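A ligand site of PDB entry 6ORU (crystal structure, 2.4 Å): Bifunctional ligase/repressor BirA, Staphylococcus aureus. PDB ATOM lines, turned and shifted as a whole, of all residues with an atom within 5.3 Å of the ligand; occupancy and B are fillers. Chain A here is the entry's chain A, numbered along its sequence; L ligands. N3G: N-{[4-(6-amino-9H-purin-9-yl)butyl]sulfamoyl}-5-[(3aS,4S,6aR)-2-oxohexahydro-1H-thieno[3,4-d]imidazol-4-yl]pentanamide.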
ATOM      1  N   SER A  93      -2.569  13.527 -15.109  1.00  0.00           N
ATOM      2  CA  SER A  93      -1.545  13.969 -14.185  1.00  0.00           C
ATOM      3  C   SER A  93      -0.445  12.924 -14.108  1.00  0.00           C
ATOM      4  O   SER A  93      -0.734  11.743 -13.878  1.00  0.00           O
ATOM      5  CB  SER A  93      -2.121  14.218 -12.780  1.00  0.00           C
ATOM      6  OG  SER A  93      -1.055  14.478 -11.870  1.00  0.00           O
ATOM      7  N   THR A  94       0.805  13.345 -14.329  1.00  0.00           N
ATOM      8  CA  THR A  94       1.921  12.420 -14.168  1.00  0.00           C
ATOM      9  C   THR A  94       1.982  11.857 -12.749  1.00  0.00           C
ATOM     10  O   THR A  94       2.436  10.716 -12.552  1.00  0.00           O
ATOM     11  CB  THR A  94       3.234  13.130 -14.494  1.00  0.00           C
ATOM     12  OG1 THR A  94       3.466  14.140 -13.516  1.00  0.00           O
ATOM     13  CG2 THR A  94       3.184  13.767 -15.855  1.00  0.00           C
ATOM     14  N   GLN A  95       1.513  12.619 -11.752  1.00  0.00           N
ATOM     15  CA  GLN A  95       1.482  12.103 -10.383  1.00  0.00           C
ATOM     16  C   GLN A  95       0.479  10.965 -10.233  1.00  0.00           C
ATOM     17  O   GLN A  95       0.753   9.964  -9.558  1.00  0.00           O
ATOM     18  CB  GLN A  95       1.151  13.220  -9.389  1.00  0.00           C
ATOM     19  CG  GLN A  95       1.512  12.860  -7.966  1.00  0.00           C
ATOM     20  CD  GLN A  95       3.004  13.127  -7.649  1.00  0.00           C
ATOM     21  OE1 GLN A  95       3.840  13.226  -8.551  1.00  0.00           O
ATOM     22  NE2 GLN A  95       3.325  13.254  -6.369  1.00  0.00           N
ATOM     23  N   GLN A 116      -0.810  18.363 -18.971  1.00  0.00           N
ATOM     24  CA  GLN A 116      -1.649  17.743 -17.954  1.00  0.00           C
ATOM     25  C   GLN A 116      -3.013  18.415 -18.005  1.00  0.00           C
ATOM     26  O   GLN A 116      -3.104  19.642 -18.096  1.00  0.00           O
ATOM     27  CB  GLN A 116      -1.037  17.864 -16.561  1.00  0.00           C
ATOM     28  CG  GLN A 116       0.344  17.240 -16.432  1.00  0.00           C
ATOM     29  CD  GLN A 116       0.863  17.216 -14.989  1.00  0.00           C
ATOM     30  OE1 GLN A 116       1.221  16.159 -14.464  1.00  0.00           O
ATOM     31  NE2 GLN A 116       0.910  18.388 -14.367  1.00  0.00           N
ATOM     32  N   LYS A 118      -5.253  17.761 -15.499  1.00  0.00           N
ATOM     33  CA  LYS A 118      -5.723  17.810 -14.127  1.00  0.00           C
ATOM     34  C   LYS A 118      -4.498  17.862 -13.212  1.00  0.00           C
ATOM     35  O   LYS A 118      -4.369  17.114 -12.243  1.00  0.00           O
ATOM     36  CB  LYS A 118      -6.628  16.618 -13.801  1.00  0.00           C
ATOM     37  CG  LYS A 118      -7.438  16.755 -12.520  1.00  0.00           C
ATOM     38  CD  LYS A 118      -7.769  15.382 -11.943  1.00  0.00           C
ATOM     39  CE  LYS A 118      -9.263  15.160 -11.701  1.00  0.00           C
ATOM     40  NZ  LYS A 118      -9.520  13.864 -11.000  1.00  0.00           N
ATOM     41  N   GLY A 119      -3.552  18.735 -13.545  1.00  0.00           N
ATOM     42  CA  GLY A 119      -2.403  18.906 -12.691  1.00  0.00           C
ATOM     43  C   GLY A 119      -2.826  19.443 -11.337  1.00  0.00           C
ATOM     44  O   GLY A 119      -3.701  20.309 -11.228  1.00  0.00           O
ATOM     45  N   ARG A 120      -2.208  18.913 -10.298  1.00  0.00           N
ATOM     46  CA  ARG A 120      -2.533  19.278  -8.927  1.00  0.00           C
ATOM     47  C   ARG A 120      -1.262  19.552  -8.165  1.00  0.00           C
ATOM     48  O   ARG A 120      -0.295  18.793  -8.262  1.00  0.00           O
ATOM     49  CB  ARG A 120      -3.333  18.182  -8.244  1.00  0.00           C
ATOM     50  CG  ARG A 120      -4.725  17.991  -8.828  1.00  0.00           C
ATOM     51  CD  ARG A 120      -5.578  19.241  -8.616  1.00  0.00           C
ATOM     52  NE  ARG A 120      -7.003  18.990  -8.817  1.00  0.00           N
ATOM     53  CZ  ARG A 120      -7.628  19.198  -9.966  1.00  0.00           C
ATOM     54  NH1 ARG A 120      -6.949  19.647 -11.023  1.00  0.00           N
ATOM     55  NH2 ARG A 120      -8.931  18.965 -10.064  1.00  0.00           N
ATOM     56  N   GLY A 121      -1.262  20.642  -7.411  1.00  0.00           N
ATOM     57  CA  GLY A 121      -0.229  20.950  -6.449  1.00  0.00           C
ATOM     58  C   GLY A 121      -0.570  20.498  -5.047  1.00  0.00           C
ATOM     59  O   GLY A 121      -1.346  19.570  -4.832  1.00  0.00           O
ATOM     60  N   ARG A 122       0.058  21.156  -4.069  1.00  0.00           N
ATOM     61  CA  ARG A 122      -0.204  20.840  -2.673  1.00  0.00           C
ATOM     62  C   ARG A 122      -1.637  21.201  -2.330  1.00  0.00           C
ATOM     63  O   ARG A 122      -2.200  22.175  -2.865  1.00  0.00           O
ATOM     64  CB  ARG A 122       0.754  21.602  -1.757  1.00  0.00           C
ATOM     65  CG  ARG A 122       2.205  21.216  -1.936  1.00  0.00           C
ATOM     66  CD  ARG A 122       3.106  22.126  -1.101  1.00  0.00           C
ATOM     67  NE  ARG A 122       2.827  22.066   0.328  1.00  0.00           N
ATOM     68  CZ  ARG A 122       3.256  22.972   1.197  1.00  0.00           C
ATOM     69  NH1 ARG A 122       3.985  23.990   0.770  1.00  0.00           N
ATOM     70  NH2 ARG A 122       2.971  22.868   2.495  1.00  0.00           N
ATOM     71  N   PHE A 123      -2.235  20.410  -1.436  1.00  0.00           N
ATOM     72  CA  PHE A 123      -3.604  20.628  -0.994  1.00  0.00           C
ATOM     73  C   PHE A 123      -4.587  20.607  -2.160  1.00  0.00           C
ATOM     74  O   PHE A 123      -5.636  21.264  -2.127  1.00  0.00           O
ATOM     75  CB  PHE A 123      -3.733  21.948  -0.209  1.00  0.00           C
ATOM     76  CG  PHE A 123      -2.740  22.095   0.913  1.00  0.00           C
ATOM     77  CD1 PHE A 123      -2.982  21.502   2.146  1.00  0.00           C
ATOM     78  CD2 PHE A 123      -1.589  22.855   0.749  1.00  0.00           C
ATOM     79  CE1 PHE A 123      -2.094  21.649   3.208  1.00  0.00           C
ATOM     80  CE2 PHE A 123      -0.681  23.003   1.802  1.00  0.00           C
ATOM     81  CZ  PHE A 123      -0.934  22.386   3.027  1.00  0.00           C
ATOM     82  N   ARG A 125      -4.461  22.039  -4.921  1.00  0.00           N
ATOM     83  CA  ARG A 125      -4.597  23.282  -5.680  1.00  0.00           C
ATOM     84  C   ARG A 125      -4.306  23.026  -7.150  1.00  0.00           C
ATOM     85  O   ARG A 125      -3.414  22.267  -7.516  1.00  0.00           O
ATOM     86  CB  ARG A 125      -3.644  24.351  -5.138  1.00  0.00           C
ATOM     87  CG  ARG A 125      -3.997  24.899  -3.747  1.00  0.00           C
ATOM     88  CD  ARG A 125      -2.724  25.495  -3.171  1.00  0.00           C
ATOM     89  NE  ARG A 125      -2.878  25.948  -1.802  1.00  0.00           N
ATOM     90  CZ  ARG A 125      -1.881  26.105  -0.949  1.00  0.00           C
ATOM     91  NH1 ARG A 125      -0.620  25.827  -1.323  1.00  0.00           N
ATOM     92  NH2 ARG A 125      -2.135  26.536   0.274  1.00  0.00           N
ATOM     93  N   HIS A 126      -5.087  23.667  -8.004  1.00  0.00           N
ATOM     94  CA  HIS A 126      -4.931  23.493  -9.439  1.00  0.00           C
ATOM     95  C   HIS A 126      -3.520  23.888  -9.865  1.00  0.00           C
ATOM     96  O   HIS A 126      -2.951  24.876  -9.386  1.00  0.00           O
ATOM     97  CB  HIS A 126      -5.994  24.336 -10.154  1.00  0.00           C
ATOM     98  CG  HIS A 126      -5.725  24.522 -11.617  1.00  0.00           C
ATOM     99  ND1 HIS A 126      -5.687  23.467 -12.504  1.00  0.00           N
ATOM    100  CD2 HIS A 126      -5.497  25.636 -12.348  1.00  0.00           C
ATOM    101  CE1 HIS A 126      -5.436  23.916 -13.718  1.00  0.00           C
ATOM    102  NE2 HIS A 126      -5.327  25.235 -13.652  1.00  0.00           N
ATOM    103  N   TRP A 127      -2.926  23.103 -10.766  1.00  0.00           N
ATOM    104  CA  TRP A 127      -1.627  23.428 -11.348  1.00  0.00           C
ATOM    105  C   TRP A 127      -1.754  23.527 -12.868  1.00  0.00           C
ATOM    106  O   TRP A 127      -2.168  22.569 -13.538  1.00  0.00           O
ATOM    107  CB  TRP A 127      -0.575  22.381 -10.963  1.00  0.00           C
ATOM    108  CG  TRP A 127       0.777  22.713 -11.524  1.00  0.00           C
ATOM    109  CD1 TRP A 127       1.288  22.304 -12.736  1.00  0.00           C
ATOM    110  CD2 TRP A 127       1.772  23.532 -10.922  1.00  0.00           C
ATOM    111  NE1 TRP A 127       2.558  22.820 -12.898  1.00  0.00           N
ATOM    112  CE2 TRP A 127       2.878  23.580 -11.811  1.00  0.00           C
ATOM    113  CE3 TRP A 127       1.854  24.234  -9.703  1.00  0.00           C
ATOM    114  CZ2 TRP A 127       4.044  24.295 -11.515  1.00  0.00           C
ATOM    115  CZ3 TRP A 127       3.016  24.951  -9.428  1.00  0.00           C
ATOM    116  CH2 TRP A 127       4.089  24.974 -10.317  1.00  0.00           C
ATOM    117  N   SER A 128      -1.380  24.694 -13.415  1.00  0.00           N
ATOM    118  CA  SER A 128      -1.441  24.956 -14.853  1.00  0.00           C
ATOM    119  C   SER A 128      -0.272  24.280 -15.550  1.00  0.00           C
ATOM    120  O   SER A 128       0.889  24.595 -15.265  1.00  0.00           O
ATOM    121  CB  SER A 128      -1.413  26.456 -15.113  1.00  0.00           C
ATOM    122  OG  SER A 128      -2.698  27.043 -15.013  1.00  0.00           O
ATOM    123  N   SER A 129      -0.579  23.390 -16.498  1.00  0.00           N
ATOM    124  CA  SER A 129       0.431  22.607 -17.202  1.00  0.00           C
ATOM    125  C   SER A 129       0.309  22.865 -18.705  1.00  0.00           C
ATOM    126  O   SER A 129      -0.154  21.989 -19.446  1.00  0.00           O
ATOM    127  CB  SER A 129       0.263  21.147 -16.900  1.00  0.00           C
ATOM    128  OG  SER A 129       0.000  20.972 -15.524  1.00  0.00           O
ATOM    129  N   LEU A 135       7.985  21.528 -17.948  1.00  0.00           N
ATOM    130  CA  LEU A 135       8.357  20.162 -17.605  1.00  0.00           C
ATOM    131  C   LEU A 135       7.441  19.692 -16.477  1.00  0.00           C
ATOM    132  O   LEU A 135       7.527  20.187 -15.339  1.00  0.00           O
ATOM    133  CB  LEU A 135       9.836  20.096 -17.220  1.00  0.00           C
ATOM    134  CG  LEU A 135      10.517  18.764 -16.903  1.00  0.00           C
ATOM    135  CD1 LEU A 135      11.998  18.917 -17.170  1.00  0.00           C
ATOM    136  CD2 LEU A 135      10.303  18.346 -15.451  1.00  0.00           C
ATOM    137  N   TRP A 136       6.542  18.762 -16.810  1.00  0.00           N
ATOM    138  CA  TRP A 136       5.595  18.157 -15.892  1.00  0.00           C
ATOM    139  C   TRP A 136       6.003  16.700 -15.702  1.00  0.00           C
ATOM    140  O   TRP A 136       5.836  15.882 -16.610  1.00  0.00           O
ATOM    141  CB  TRP A 136       4.162  18.260 -16.427  1.00  0.00           C
ATOM    142  CG  TRP A 136       3.877  19.502 -17.251  1.00  0.00           C
ATOM    143  CD1 TRP A 136       3.376  19.549 -18.526  1.00  0.00           C
ATOM    144  CD2 TRP A 136       4.066  20.869 -16.845  1.00  0.00           C
ATOM    145  NE1 TRP A 136       3.233  20.862 -18.930  1.00  0.00           N
ATOM    146  CE2 TRP A 136       3.652  21.692 -17.923  1.00  0.00           C
ATOM    147  CE3 TRP A 136       4.545  21.485 -15.675  1.00  0.00           C
ATOM    148  CZ2 TRP A 136       3.701  23.084 -17.862  1.00  0.00           C
ATOM    149  CZ3 TRP A 136       4.594  22.858 -15.628  1.00  0.00           C
ATOM    150  CH2 TRP A 136       4.174  23.645 -16.712  1.00  0.00           C
ATOM    151  N   MET A 137       6.497  16.374 -14.520  1.00  0.00           N
ATOM    152  CA  MET A 137       7.135  15.093 -14.332  1.00  0.00           C
ATOM    153  C   MET A 137       6.939  14.618 -12.889  1.00  0.00           C
ATOM    154  O   MET A 137       6.854  15.431 -11.955  1.00  0.00           O
ATOM    155  CB  MET A 137       8.620  15.195 -14.719  1.00  0.00           C
ATOM    156  CG  MET A 137       9.540  14.178 -14.106  1.00  0.00           C
ATOM    157  SD  MET A 137      11.212  14.247 -14.764  1.00  0.00           S
ATOM    158  CE  MET A 137      11.985  15.284 -13.489  1.00  0.00           C
ATOM    159  N   SER A 138       6.843  13.306 -12.732  1.00  0.00           N
ATOM    160  CA  SER A 138       6.768  12.668 -11.423  1.00  0.00           C
ATOM    161  C   SER A 138       7.854  11.609 -11.335  1.00  0.00           C
ATOM    162  O   SER A 138       8.024  10.809 -12.262  1.00  0.00           O
ATOM    163  CB  SER A 138       5.381  12.066 -11.178  1.00  0.00           C
ATOM    164  OG  SER A 138       4.401  13.097 -11.149  1.00  0.00           O
ATOM    165  N   ASN A 179       9.072  23.900  -0.769  1.00  0.00           N
ATOM    166  CA  ASN A 179       8.950  23.204  -2.067  1.00  0.00           C
ATOM    167  C   ASN A 179       8.614  24.168  -3.209  1.00  0.00           C
ATOM    168  O   ASN A 179       7.832  23.832  -4.102  1.00  0.00           O
ATOM    169  CB  ASN A 179       7.906  22.087  -1.989  1.00  0.00           C
ATOM    170  CG  ASN A 179       6.773  22.434  -1.073  1.00  0.00           C
ATOM    171  OD1 ASN A 179       5.963  23.316  -1.366  1.00  0.00           O
ATOM    172  ND2 ASN A 179       6.732  21.760   0.074  1.00  0.00           N
ATOM    173  N   ASP A 180       9.250  25.327  -3.216  1.00  0.00           N
ATOM    174  CA  ASP A 180       9.082  26.322  -4.268  1.00  0.00           C
ATOM    175  C   ASP A 180      10.459  26.771  -4.747  1.00  0.00           C
ATOM    176  O   ASP A 180      11.352  26.995  -3.936  1.00  0.00           O
ATOM    177  CB  ASP A 180       8.319  27.567  -3.768  1.00  0.00           C
ATOM    178  CG  ASP A 180       6.837  27.326  -3.535  1.00  0.00           C
ATOM    179  OD1 ASP A 180       6.365  26.180  -3.612  1.00  0.00           O
ATOM    180  OD2 ASP A 180       6.127  28.313  -3.277  1.00  0.00           O
ATOM    181  N   LYS A 187       7.535  32.508  -9.205  1.00  0.00           N
ATOM    182  CA  LYS A 187       7.617  31.063  -9.000  1.00  0.00           C
ATOM    183  C   LYS A 187       7.862  30.387 -10.341  1.00  0.00           C
ATOM    184  O   LYS A 187       7.006  30.432 -11.239  1.00  0.00           O
ATOM    185  CB  LYS A 187       6.342  30.545  -8.350  1.00  0.00           C
ATOM    186  CG  LYS A 187       6.320  29.013  -8.148  1.00  0.00           C
ATOM    187  CD  LYS A 187       5.281  28.623  -7.117  1.00  0.00           C
ATOM    188  CE  LYS A 187       5.183  27.118  -6.906  1.00  0.00           C
ATOM    189  NZ  LYS A 187       4.607  26.861  -5.531  1.00  0.00           N
ATOM    190  N   CYS A 189       9.092  27.034 -10.278  1.00  0.00           N
ATOM    191  CA  CYS A 189       8.897  25.609 -10.059  1.00  0.00           C
ATOM    192  C   CYS A 189       8.246  25.374  -8.707  1.00  0.00           C
ATOM    193  O   CYS A 189       8.554  26.061  -7.724  1.00  0.00           O
ATOM    194  CB  CYS A 189      10.200  24.835 -10.127  1.00  0.00           C
ATOM    195  SG  CYS A 189      10.092  23.195  -9.398  1.00  0.00           S
ATOM    196  N   GLY A 190       7.362  24.398  -8.671  1.00  0.00           N
ATOM    197  CA  GLY A 190       6.953  23.812  -7.407  1.00  0.00           C
ATOM    198  C   GLY A 190       6.957  22.310  -7.515  1.00  0.00           C
ATOM    199  O   GLY A 190       6.767  21.747  -8.596  1.00  0.00           O
ATOM    200  N   PHE A 191       7.199  21.657  -6.388  1.00  0.00           N
ATOM    201  CA  PHE A 191       7.235  20.210  -6.371  1.00  0.00           C
ATOM    202  C   PHE A 191       6.524  19.708  -5.119  1.00  0.00           C
ATOM    203  O   PHE A 191       6.266  20.449  -4.178  1.00  0.00           O
ATOM    204  CB  PHE A 191       8.663  19.655  -6.485  1.00  0.00           C
ATOM    205  CG  PHE A 191       9.579  20.063  -5.353  1.00  0.00           C
ATOM    206  CD1 PHE A 191      10.209  21.316  -5.361  1.00  0.00           C
ATOM    207  CD2 PHE A 191       9.855  19.196  -4.305  1.00  0.00           C
ATOM    208  CE1 PHE A 191      11.068  21.693  -4.320  1.00  0.00           C
ATOM    209  CE2 PHE A 191      10.719  19.566  -3.276  1.00  0.00           C
ATOM    210  CZ  PHE A 191      11.317  20.818  -3.281  1.00  0.00           C
ATOM    211  N   LEU A 192       6.161  18.449  -5.150  1.00  0.00           N
ATOM    212  CA  LEU A 192       5.318  17.869  -4.124  1.00  0.00           C
ATOM    213  C   LEU A 192       5.772  16.432  -3.960  1.00  0.00           C
ATOM    214  O   LEU A 192       5.891  15.701  -4.940  1.00  0.00           O
ATOM    215  CB  LEU A 192       3.843  17.933  -4.533  1.00  0.00           C
ATOM    216  CG  LEU A 192       2.892  16.959  -3.859  1.00  0.00           C
ATOM    217  CD1 LEU A 192       2.582  17.406  -2.435  1.00  0.00           C
ATOM    218  CD2 LEU A 192       1.629  16.914  -4.669  1.00  0.00           C
ATOM    219  N   GLY A 208       6.442  14.970  -7.445  1.00  0.00           N
ATOM    220  CA  GLY A 208       5.857  15.637  -8.586  1.00  0.00           C
ATOM    221  C   GLY A 208       6.493  16.987  -8.830  1.00  0.00           C
ATOM    222  O   GLY A 208       6.364  17.880  -7.991  1.00  0.00           O
ATOM    223  N   ILE A 209       7.156  17.160  -9.978  1.00  0.00           N
ATOM    224  CA  ILE A 209       7.930  18.370 -10.280  1.00  0.00           C
ATOM    225  C   ILE A 209       7.325  19.077 -11.487  1.00  0.00           C
ATOM    226  O   ILE A 209       7.263  18.514 -12.586  1.00  0.00           O
ATOM    227  CB  ILE A 209       9.400  18.038 -10.523  1.00  0.00           C
ATOM    228  CG1 ILE A 209      10.006  17.369  -9.287  1.00  0.00           C
ATOM    229  CG2 ILE A 209      10.172  19.301 -10.881  1.00  0.00           C
ATOM    230  CD1 ILE A 209      11.402  16.856  -9.473  1.00  0.00           C
ATOM    231  N   GLY A 210       6.902  20.331 -11.291  1.00  0.00           N
ATOM    232  CA  GLY A 210       6.449  21.190 -12.367  1.00  0.00           C
ATOM    233  C   GLY A 210       7.339  22.400 -12.511  1.00  0.00           C
ATOM    234  O   GLY A 210       7.507  23.169 -11.560  1.00  0.00           O
ATOM    235  N   ASN A 212       8.225  25.721 -15.079  1.00  0.00           N
ATOM    236  CA  ASN A 212       7.840  26.521 -16.228  1.00  0.00           C
ATOM    237  C   ASN A 212       9.074  26.777 -17.091  1.00  0.00           C
ATOM    238  O   ASN A 212      10.033  27.407 -16.629  1.00  0.00           O
ATOM    239  CB  ASN A 212       7.224  27.839 -15.749  1.00  0.00           C
ATOM    240  CG  ASN A 212       6.069  27.628 -14.775  1.00  0.00           C
ATOM    241  OD1 ASN A 212       5.125  26.878 -15.057  1.00  0.00           O
ATOM    242  ND2 ASN A 212       6.136  28.302 -13.619  1.00  0.00           N
ATOM    243  N   GLN A 215       7.123  29.684 -20.896  1.00  0.00           N
ATOM    244  CA  GLN A 215       5.917  30.518 -20.903  1.00  0.00           C
ATOM    245  C   GLN A 215       6.281  31.974 -21.123  1.00  0.00           C
ATOM    246  O   GLN A 215       7.150  32.532 -20.447  1.00  0.00           O
ATOM    247  CB  GLN A 215       5.144  30.383 -19.587  1.00  0.00           C
ATOM    248  CG  GLN A 215       4.334  29.120 -19.432  1.00  0.00           C
ATOM    249  CD  GLN A 215       5.083  28.089 -18.629  1.00  0.00           C
ATOM    250  OE1 GLN A 215       6.319  28.043 -18.682  1.00  0.00           O
ATOM    251  NE2 GLN A 215       4.355  27.259 -17.885  1.00  0.00           N
ATOM    252  N   PHE A 220       0.550  32.708 -18.826  1.00  0.00           N
ATOM    253  CA  PHE A 220       0.063  32.418 -17.486  1.00  0.00           C
ATOM    254  C   PHE A 220      -1.325  33.025 -17.293  1.00  0.00           C
ATOM    255  O   PHE A 220      -1.614  34.112 -17.813  1.00  0.00           O
ATOM    256  CB  PHE A 220       1.018  32.993 -16.436  1.00  0.00           C
ATOM    257  CG  PHE A 220       2.329  32.247 -16.335  1.00  0.00           C
ATOM    258  CD1 PHE A 220       2.371  30.938 -15.891  1.00  0.00           C
ATOM    259  CD2 PHE A 220       3.527  32.884 -16.642  1.00  0.00           C
ATOM    260  CE1 PHE A 220       3.579  30.260 -15.784  1.00  0.00           C
ATOM    261  CE2 PHE A 220       4.738  32.209 -16.527  1.00  0.00           C
ATOM    262  CZ  PHE A 220       4.772  30.899 -16.114  1.00  0.00           C
ATOM    263  N   ILE A 224      -2.199  34.261 -11.734  1.00  0.00           N
ATOM    264  CA  ILE A 224      -0.877  33.878 -11.263  1.00  0.00           C
ATOM    265  C   ILE A 224       0.242  34.636 -11.966  1.00  0.00           C
ATOM    266  O   ILE A 224       1.417  34.347 -11.713  1.00  0.00           O
ATOM    267  CB  ILE A 224      -0.653  32.351 -11.383  1.00  0.00           C
ATOM    268  CG1 ILE A 224      -0.655  31.927 -12.849  1.00  0.00           C
ATOM    269  CG2 ILE A 224      -1.703  31.579 -10.599  1.00  0.00           C
ATOM    270  CD1 ILE A 224      -0.057  30.576 -13.066  1.00  0.00           C
ATOM    271  N   ARG A 227       3.009  36.253 -10.002  1.00  0.00           N
ATOM    272  CA  ARG A 227       3.731  35.346  -9.111  1.00  0.00           C
ATOM    273  C   ARG A 227       4.298  34.128  -9.828  1.00  0.00           C
ATOM    274  O   ARG A 227       4.844  33.250  -9.164  1.00  0.00           O
ATOM    275  CB  ARG A 227       2.823  34.859  -7.968  1.00  0.00           C
ATOM    276  CG  ARG A 227       1.837  35.862  -7.454  1.00  0.00           C
ATOM    277  CD  ARG A 227       1.229  35.420  -6.118  1.00  0.00           C
ATOM    278  NE  ARG A 227       2.239  35.053  -5.121  1.00  0.00           N
ATOM    279  CZ  ARG A 227       3.037  35.908  -4.476  1.00  0.00           C
ATOM    280  NH1 ARG A 227       3.926  35.431  -3.604  1.00  0.00           N
ATOM    281  NH2 ARG A 227       2.954  37.222  -4.686  1.00  0.00           N
ATOM    282  N   ALA A 228       4.177  34.044 -11.139  1.00  0.00           N
ATOM    283  CA  ALA A 228       4.736  32.936 -11.897  1.00  0.00           C
ATOM    284  C   ALA A 228       5.731  33.451 -12.914  1.00  0.00           C
ATOM    285  O   ALA A 228       5.585  34.556 -13.430  1.00  0.00           O
ATOM    286  CB  ALA A 228       3.647  32.125 -12.625  1.00  0.00           C
HETATM  287  C21 N3G L   1      -0.570  27.071 -10.706  1.00  0.00           C
HETATM  288  C24 N3G L   1       2.467  27.214 -12.749  1.00  0.00           C
HETATM  289  C18 N3G L   1      -0.555  27.725  -7.619  1.00  0.00           C
HETATM  290  C19 N3G L   1      -0.178  28.670  -8.725  1.00  0.00           C
HETATM  291  C23 N3G L   1       1.330  27.267 -11.841  1.00  0.00           C
HETATM  292  C27 N3G L   1       3.538  28.758 -11.314  1.00  0.00           C
HETATM  293  C29 N3G L   1       1.427  28.112 -10.719  1.00  0.00           C
HETATM  294  C30 N3G L   1       3.099  17.671 -10.158  1.00  0.00           C
HETATM  295  C32 N3G L   1       0.969  17.061 -10.940  1.00  0.00           C
HETATM  296  C01 N3G L   1       3.226  16.571 -11.283  1.00  0.00           C
HETATM  297  C02 N3G L   1       3.896  17.275 -12.460  1.00  0.00           C
HETATM  298  C04 N3G L   1       3.784  18.999 -10.575  1.00  0.00           C
HETATM  299  C05 N3G L   1       3.276  20.322  -9.934  1.00  0.00           C
HETATM  300  C06 N3G L   1       3.675  20.549  -8.415  1.00  0.00           C
HETATM  301  C07 N3G L   1       2.732  21.513  -7.660  1.00  0.00           C
HETATM  302  C08 N3G L   1       3.060  22.037  -6.172  1.00  0.00           C
HETATM  303  C09 N3G L   1       3.389  23.553  -6.137  1.00  0.00           C
HETATM  304  C16 N3G L   1       0.174  25.679  -6.359  1.00  0.00           C
HETATM  305  C17 N3G L   1       0.597  26.954  -7.028  1.00  0.00           C
HETATM  306  N11 N3G L   1       2.802  24.634  -5.448  1.00  0.00           N
HETATM  307  N15 N3G L   1       0.536  25.673  -4.951  1.00  0.00           N
HETATM  308  N20 N3G L   1       0.229  27.994  -9.995  1.00  0.00           N
HETATM  309  N22 N3G L   1       0.064  26.631 -11.817  1.00  0.00           N
HETATM  310  N25 N3G L   1       2.544  26.441 -13.879  1.00  0.00           N
HETATM  311  N26 N3G L   1       3.566  27.982 -12.457  1.00  0.00           N
HETATM  312  N28 N3G L   1       2.537  28.860 -10.436  1.00  0.00           N
HETATM  313  N31 N3G L   1       1.720  17.836 -10.071  1.00  0.00           N
HETATM  314  N34 N3G L   1       1.862  16.259 -11.680  1.00  0.00           N
HETATM  315  O10 N3G L   1       4.247  23.970  -6.862  1.00  0.00           O
HETATM  316  O13 N3G L   1       2.203  25.101  -3.187  1.00  0.00           O
HETATM  317  O14 N3G L   1       0.951  23.398  -4.312  1.00  0.00           O
HETATM  318  O33 N3G L   1      -0.259  17.004 -11.081  1.00  0.00           O
HETATM  319  S03 N3G L   1       3.483  18.999 -12.363  1.00  0.00           S
HETATM  320  S12 N3G L   1       1.602  24.647  -4.361  1.00  0.00           S
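Gln 95 touches the ligand. CA of Gly 119 touches O33 of the ligand (3.3 Å). CA of Gly 121 touches C07 of the ligand, 3.2 Å away. His 126 touches the ligand (O to C21, 3.5 Å). Trp 127 touches the ligand (CZ3 to O10, 3.0 Å). C of Trp 136 touches C02 of the ligand (3.9 Å). Met 137 touches the ligand. Ser 138 touches the ligand. Gly 190 touches the ligand. N of Phe 191 touches O10 of the ligand, 3.8 Å away. Gly 208 touches the ligand. Ile 209 touches the ligand. Gly 210 touches the ligand. CD1 of Ile 224 touches C29 of the ligand, at 3.7 Å. CB of Ala 228 touches C27 of the ligand, 3.6 Å away. Hydrophobic or aromatic side chains that line the ligand: Trp 127, Ile 224 and Ala 228.
The backbone NH (N) of Arg 122 lies within hydrogen-bond range of an oxygen (O14) of the ligand (2.4 Å). The backbone carbonyl oxygen (O) of Arg 120 is in hydrogen-bond range of a nitrogen (N31) of the ligand (2.9 Å). The backbone NH (N) of Ser 128 lies within hydrogen-bond range of a nitrogen (N22) of the ligand, at 2.9 Å. OG1 of Thr 94 lies within hydrogen-bond range of N34 of the ligand (3.2 Å). The backbone NH (N) of Arg 120 lies within hydrogen-bond range of an oxygen (O33) of the ligand, at 2.8 Å. The side-chain amide oxygen (OE1) of Gln 116 sits at hydrogen-bond distance from a nitrogen (N34) of the ligand (2.9 Å). OG of Ser 93 lies within hydrogen-bond range of O33 of the ligand (2.8 Å). NH1 of Arg 125 sits at hydrogen-bond distance from O13 of the ligand (3.5 Å). The backbone carbonyl oxygen (O) of Ser 128 sits at hydrogen-bond distance from a nitrogen (N25) of the ligand. The side-chain amino group (NZ) of Lys 187 lies within hydrogen-bond range of a nitrogen (N11) of the ligand (2.9 Å). ND2 of Asn 212 is in hydrogen-bond range of N26 of the ligand (2.8 Å).
The side-chain sulfur (SG) of Cys 189 sits close to the backbone carbonyl oxygen (O) of Gly 210 (3.4 Å). The side-chain hydroxyl of Ser 93 sits close to the backbone NH of Gln 95 (3.2 Å). N of Lys 187 lies within hydrogen-bond range of O of Arg 227 (2.8 Å). The side-chain hydroxyl (OG) of Ser 138 lies within hydrogen-bond range of the side-chain amide oxygen (OE1) of Gln 95, 2.7 Å away. O of Leu 192 is in hydrogen-bond range of N of Gly 208. NE2 of Gln 215 is in hydrogen-bond range of OD1 of Asn 212. The side-chain hydroxyl (OG) of Ser 129 lies within hydrogen-bond range of the side-chain amide nitrogen (NE2) of Gln 116, 3.0 Å away. The side-chain amide oxygen of Asn 179 is in hydrogen-bond range of the guanidinium group of Arg 122, 3.0 Å away.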
